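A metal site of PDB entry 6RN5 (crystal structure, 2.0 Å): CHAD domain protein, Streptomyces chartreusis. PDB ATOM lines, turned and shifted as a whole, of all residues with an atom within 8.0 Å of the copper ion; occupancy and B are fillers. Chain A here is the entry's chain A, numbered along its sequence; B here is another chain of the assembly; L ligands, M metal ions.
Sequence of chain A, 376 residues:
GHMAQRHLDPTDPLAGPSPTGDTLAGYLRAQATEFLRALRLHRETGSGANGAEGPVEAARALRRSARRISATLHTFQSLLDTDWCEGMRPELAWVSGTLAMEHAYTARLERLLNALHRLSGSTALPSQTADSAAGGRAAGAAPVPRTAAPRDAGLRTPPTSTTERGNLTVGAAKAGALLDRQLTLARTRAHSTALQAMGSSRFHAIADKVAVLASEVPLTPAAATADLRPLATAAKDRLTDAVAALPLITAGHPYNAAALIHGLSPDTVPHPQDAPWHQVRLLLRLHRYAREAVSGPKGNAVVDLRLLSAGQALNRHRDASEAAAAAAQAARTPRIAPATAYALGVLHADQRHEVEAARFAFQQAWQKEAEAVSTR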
ATOM      1  N   ALA A 258     -32.797   0.810  -4.991  1.00  0.00           N
ATOM      2  CA  ALA A 258     -32.187  -0.395  -4.440  1.00  0.00           C
ATOM      3  C   ALA A 258     -31.095  -0.116  -3.368  1.00  0.00           C
ATOM      4  O   ALA A 258     -30.898  -0.939  -2.467  1.00  0.00           O
ATOM      5  CB  ALA A 258     -31.630  -1.256  -5.586  1.00  0.00           C
ATOM      6  N   ALA A 259     -30.407   1.024  -3.467  1.00  0.00           N
ATOM      7  CA  ALA A 259     -29.221   1.337  -2.634  1.00  0.00           C
ATOM      8  C   ALA A 259     -28.107   0.276  -2.719  1.00  0.00           C
ATOM      9  O   ALA A 259     -27.713  -0.401  -1.744  1.00  0.00           O
ATOM     10  CB  ALA A 259     -29.599   1.603  -1.196  1.00  0.00           C
ATOM     11  N   LEU A 260     -27.569   0.165  -3.912  1.00  0.00           N
ATOM     12  CA  LEU A 260     -26.520  -0.790  -4.194  1.00  0.00           C
ATOM     13  C   LEU A 260     -25.125  -0.259  -3.859  1.00  0.00           C
ATOM     14  O   LEU A 260     -24.201  -1.028  -3.613  1.00  0.00           O
ATOM     15  CB  LEU A 260     -26.624  -1.220  -5.642  1.00  0.00           C
ATOM     16  CG  LEU A 260     -28.000  -1.782  -5.971  1.00  0.00           C
ATOM     17  CD1 LEU A 260     -28.129  -2.078  -7.454  1.00  0.00           C
ATOM     18  CD2 LEU A 260     -28.256  -3.056  -5.170  1.00  0.00           C
ATOM     19  N   ILE A 261     -24.958   1.039  -3.818  1.00  0.00           N
ATOM     20  CA  ILE A 261     -23.719   1.590  -3.328  1.00  0.00           C
ATOM     21  C   ILE A 261     -24.106   2.425  -2.142  1.00  0.00           C
ATOM     22  O   ILE A 261     -24.860   3.381  -2.278  1.00  0.00           O
ATOM     23  CB  ILE A 261     -23.017   2.468  -4.383  1.00  0.00           C
ATOM     24  CG1 ILE A 261     -22.922   1.757  -5.737  1.00  0.00           C
ATOM     25  CG2 ILE A 261     -21.609   2.781  -3.923  1.00  0.00           C
ATOM     26  CD1 ILE A 261     -22.510   2.677  -6.881  1.00  0.00           C
ATOM     27  N   HIS A 262     -23.646   2.021  -0.969  1.00  0.00           N
ATOM     28  CA  HIS A 262     -23.886   2.753   0.285  1.00  0.00           C
ATOM     29  C   HIS A 262     -22.674   2.469   1.148  1.00  0.00           C
ATOM     30  O   HIS A 262     -21.966   1.461   0.897  1.00  0.00           O
ATOM     31  CB  HIS A 262     -25.177   2.300   1.001  1.00  0.00           C
ATOM     32  CG  HIS A 262     -25.165   0.871   1.455  1.00  0.00           C
ATOM     33  ND1 HIS A 262     -24.335   0.414   2.456  1.00  0.00           N
ATOM     34  CD2 HIS A 262     -25.831  -0.214   0.997  1.00  0.00           C
ATOM     35  CE1 HIS A 262     -24.524  -0.886   2.617  1.00  0.00           C
ATOM     36  NE2 HIS A 262     -25.426  -1.285   1.745  1.00  0.00           N
ATOM     37  N   GLY A 263     -22.421   3.340   2.115  1.00  0.00           N
ATOM     38  CA  GLY A 263     -21.369   3.105   3.126  1.00  0.00           C
ATOM     39  C   GLY A 263     -21.862   2.261   4.306  1.00  0.00           C
ATOM     40  O   GLY A 263     -22.987   1.742   4.299  1.00  0.00           O
ATOM     41  N   LEU A 264     -21.046   2.154   5.345  1.00  0.00           N
ATOM     42  CA  LEU A 264     -21.369   1.272   6.458  1.00  0.00           C
ATOM     43  C   LEU A 264     -20.999   1.885   7.800  1.00  0.00           C
ATOM     44  O   LEU A 264     -19.820   2.029   8.089  1.00  0.00           O
ATOM     45  CB  LEU A 264     -20.647  -0.097   6.297  1.00  0.00           C
ATOM     46  CG  LEU A 264     -21.178  -1.204   5.361  1.00  0.00           C
ATOM     47  CD1 LEU A 264     -20.360  -2.479   5.539  1.00  0.00           C
ATOM     48  CD2 LEU A 264     -22.656  -1.527   5.577  1.00  0.00           C
ATOM     49  N   PRO A 270     -28.890   0.745   6.062  1.00  0.00           N
ATOM     50  CA  PRO A 270     -28.731   0.737   4.597  1.00  0.00           C
ATOM     51  C   PRO A 270     -29.936   0.138   3.824  1.00  0.00           C
ATOM     52  O   PRO A 270     -30.264   0.639   2.754  1.00  0.00           O
ATOM     53  CB  PRO A 270     -27.418  -0.063   4.409  1.00  0.00           C
ATOM     54  CG  PRO A 270     -27.332  -0.937   5.607  1.00  0.00           C
ATOM     55  CD  PRO A 270     -27.980  -0.202   6.736  1.00  0.00           C
ATOM     56  N   HIS A 271     -30.624  -0.836   4.402  1.00  0.00           N
ATOM     57  CA  HIS A 271     -31.718  -1.554   3.717  1.00  0.00           C
ATOM     58  C   HIS A 271     -32.927  -1.602   4.636  1.00  0.00           C
ATOM     59  O   HIS A 271     -33.243  -2.622   5.206  1.00  0.00           O
ATOM     60  CB  HIS A 271     -31.202  -2.947   3.328  1.00  0.00           C
ATOM     61  CG  HIS A 271     -30.033  -2.896   2.392  1.00  0.00           C
ATOM     62  ND1 HIS A 271     -30.163  -2.428   1.094  1.00  0.00           N
ATOM     63  CD2 HIS A 271     -28.725  -3.161   2.564  1.00  0.00           C
ATOM     64  CE1 HIS A 271     -28.995  -2.449   0.499  1.00  0.00           C
ATOM     65  NE2 HIS A 271     -28.086  -2.876   1.365  1.00  0.00           N
ATOM     66  N   ASP A 274     -35.876  -4.126   4.633  1.00  0.00           N
ATOM     67  CA  ASP A 274     -35.637  -5.505   5.092  1.00  0.00           C
ATOM     68  C   ASP A 274     -36.384  -5.801   6.410  1.00  0.00           C
ATOM     69  O   ASP A 274     -36.853  -6.924   6.587  1.00  0.00           O
ATOM     70  CB  ASP A 274     -34.137  -5.798   5.307  1.00  0.00           C
ATOM     71  CG  ASP A 274     -33.382  -6.061   3.980  1.00  0.00           C
ATOM     72  OD1 ASP A 274     -33.926  -5.860   2.886  1.00  0.00           O
ATOM     73  OD2 ASP A 274     -32.222  -6.442   4.046  1.00  0.00           O
ATOM     74  N   SER A 321     -30.142 -11.223   2.185  1.00  0.00           N
ATOM     75  CA  SER A 321     -29.883 -10.008   2.909  1.00  0.00           C
ATOM     76  C   SER A 321     -28.573 -10.076   3.704  1.00  0.00           C
ATOM     77  O   SER A 321     -27.736  -9.171   3.597  1.00  0.00           O
ATOM     78  CB  SER A 321     -31.060  -9.700   3.830  1.00  0.00           C
ATOM     79  OG  SER A 321     -30.804  -8.533   4.570  1.00  0.00           O
ATOM     80  N   ALA A 324     -25.477 -10.335   1.464  1.00  0.00           N
ATOM     81  CA  ALA A 324     -25.095  -9.074   0.863  1.00  0.00           C
ATOM     82  C   ALA A 324     -24.290  -8.248   1.870  1.00  0.00           C
ATOM     83  O   ALA A 324     -23.323  -7.605   1.478  1.00  0.00           O
ATOM     84  CB  ALA A 324     -26.320  -8.315   0.368  1.00  0.00           C
ATOM     85  N   ALA A 325     -24.693  -8.292   3.143  1.00  0.00           N
ATOM     86  CA  ALA A 325     -24.046  -7.501   4.182  1.00  0.00           C
ATOM     87  C   ALA A 325     -22.657  -8.041   4.465  1.00  0.00           C
ATOM     88  O   ALA A 325     -21.756  -7.278   4.727  1.00  0.00           O
ATOM     89  CB  ALA A 325     -24.876  -7.482   5.452  1.00  0.00           C
ATOM     90  N   ALA A 326     -22.458  -9.352   4.376  1.00  0.00           N
ATOM     91  CA  ALA A 326     -21.123  -9.884   4.532  1.00  0.00           C
ATOM     92  C   ALA A 326     -20.224  -9.437   3.370  1.00  0.00           C
ATOM     93  O   ALA A 326     -19.045  -9.219   3.575  1.00  0.00           O
ATOM     94  CB  ALA A 326     -21.136 -11.394   4.622  1.00  0.00           C
ATOM     95  N   ALA A 327     -20.744  -9.340   2.150  1.00  0.00           N
ATOM     96  CA  ALA A 327     -19.921  -8.881   1.031  1.00  0.00           C
ATOM     97  C   ALA A 327     -19.535  -7.415   1.215  1.00  0.00           C
ATOM     98  O   ALA A 327     -18.383  -7.046   1.004  1.00  0.00           O
ATOM     99  CB  ALA A 327     -20.666  -9.054  -0.269  1.00  0.00           C
ATOM    100  N   ALA A 328     -20.495  -6.583   1.616  1.00  0.00           N
ATOM    101  CA  ALA A 328     -20.219  -5.166   1.832  1.00  0.00           C
ATOM    102  C   ALA A 328     -19.142  -4.999   2.911  1.00  0.00           C
ATOM    103  O   ALA A 328     -18.149  -4.296   2.723  1.00  0.00           O
ATOM    104  CB  ALA A 328     -21.500  -4.378   2.177  1.00  0.00           C
ATOM    105  N   GLN A 329     -19.331  -5.687   4.023  1.00  0.00           N
ATOM    106  CA  GLN A 329     -18.428  -5.592   5.118  1.00  0.00           C
ATOM    107  C   GLN A 329     -17.036  -6.102   4.738  1.00  0.00           C
ATOM    108  O   GLN A 329     -16.054  -5.497   5.081  1.00  0.00           O
ATOM    109  CB  GLN A 329     -19.008  -6.325   6.356  1.00  0.00           C
ATOM    110  CG  GLN A 329     -18.176  -6.106   7.655  1.00  0.00           C
ATOM    111  CD  GLN A 329     -18.058  -4.636   8.097  1.00  0.00           C
ATOM    112  OE1 GLN A 329     -19.044  -3.883   8.109  1.00  0.00           O
ATOM    113  NE2 GLN A 329     -16.845  -4.212   8.435  1.00  0.00           N
ATOM    114  N   HIS A 348     -22.396  -8.104  -3.642  1.00  0.00           N
ATOM    115  CA  HIS A 348     -23.406  -7.417  -2.861  1.00  0.00           C
ATOM    116  C   HIS A 348     -24.625  -7.081  -3.689  1.00  0.00           C
ATOM    117  O   HIS A 348     -25.753  -7.290  -3.230  1.00  0.00           O
ATOM    118  CB  HIS A 348     -22.838  -6.135  -2.239  1.00  0.00           C
ATOM    119  CG  HIS A 348     -23.871  -5.252  -1.599  1.00  0.00           C
ATOM    120  ND1 HIS A 348     -24.518  -4.257  -2.298  1.00  0.00           N
ATOM    121  CD2 HIS A 348     -24.374  -5.237  -0.341  1.00  0.00           C
ATOM    122  CE1 HIS A 348     -25.370  -3.640  -1.473  1.00  0.00           C
ATOM    123  NE2 HIS A 348     -25.306  -4.231  -0.283  1.00  0.00           N
ATOM    124  N   ALA A 349     -24.419  -6.613  -4.909  1.00  0.00           N
ATOM    125  CA  ALA A 349     -25.516  -6.252  -5.783  1.00  0.00           C
ATOM    126  C   ALA A 349     -26.344  -7.482  -6.175  1.00  0.00           C
ATOM    127  O   ALA A 349     -27.594  -7.482  -6.100  1.00  0.00           O
ATOM    128  CB  ALA A 349     -24.974  -5.554  -7.040  1.00  0.00           C
ATOM    129  N   ARG A 352     -28.455  -8.468  -3.291  1.00  0.00           N
ATOM    130  CA  ARG A 352     -29.580  -7.558  -3.151  1.00  0.00           C
ATOM    131  C   ARG A 352     -30.633  -7.816  -4.225  1.00  0.00           C
ATOM    132  O   ARG A 352     -31.837  -7.683  -3.966  1.00  0.00           O
ATOM    133  CB  ARG A 352     -29.139  -6.098  -3.191  1.00  0.00           C
ATOM    134  CG  ARG A 352     -28.321  -5.669  -2.009  1.00  0.00           C
ATOM    135  CD  ARG A 352     -29.003  -6.010  -0.685  1.00  0.00           C
ATOM    136  NE  ARG A 352     -30.371  -5.493  -0.516  1.00  0.00           N
ATOM    137  CZ  ARG A 352     -31.115  -5.661   0.583  1.00  0.00           C
ATOM    138  NH1 ARG A 352     -30.669  -6.371   1.620  1.00  0.00           N
ATOM    139  NH2 ARG A 352     -32.327  -5.134   0.656  1.00  0.00           N
ATOM    140  N   TYR B 342     -15.249  -0.644  -5.774  1.00  0.00           N
ATOM    141  CA  TYR B 342     -16.472  -1.358  -5.442  1.00  0.00           C
ATOM    142  C   TYR B 342     -17.616  -0.702  -6.125  1.00  0.00           C
ATOM    143  O   TYR B 342     -18.428  -1.367  -6.719  1.00  0.00           O
ATOM    144  CB  TYR B 342     -16.633  -1.349  -3.915  1.00  0.00           C
ATOM    145  CG  TYR B 342     -17.921  -1.903  -3.304  1.00  0.00           C
ATOM    146  CD1 TYR B 342     -19.095  -1.111  -3.266  1.00  0.00           C
ATOM    147  CD2 TYR B 342     -17.916  -3.123  -2.673  1.00  0.00           C
ATOM    148  CE1 TYR B 342     -20.238  -1.593  -2.652  1.00  0.00           C
ATOM    149  CE2 TYR B 342     -19.049  -3.622  -2.044  1.00  0.00           C
ATOM    150  CZ  TYR B 342     -20.200  -2.845  -2.023  1.00  0.00           C
ATOM    151  OH  TYR B 342     -21.287  -3.357  -1.419  1.00  0.00           O
HETATM  152 CL1  LIG L   1     -25.682  -4.414   3.029  1.00  0.00          CL
HETATM  153 CU    CU M   1     -26.195  -3.294   1.290  1.00  0.00          CU
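Of the 21 residues printed, 3 come within 4 Å of the copper ion.
Along chain A the residues within 4 Å of the copper ion span positions 262 to 348.
The nearest printed residue that does not touch the copper ion is Arg 352 (4.4 Å).
ND1 of His 271 sits close to NE of Arg 352.
A ring nitrogen (ND1) of His 348 sits close to the side-chain hydroxyl (OH) of Tyr 342 of chain B (3.5 Å).
A ring nitrogen (NE2) of His 271 is bound to the copper ion (1.9 Å).
NE2 of His 348 binds the copper ion (2.0 Å).
The copper ion is bound by a chlorine (CL1) of the ligand, 2.1 Å away.
A ring nitrogen (NE2) of His 262 binds the copper ion.
The copper ion has four donor atoms within binding distance.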
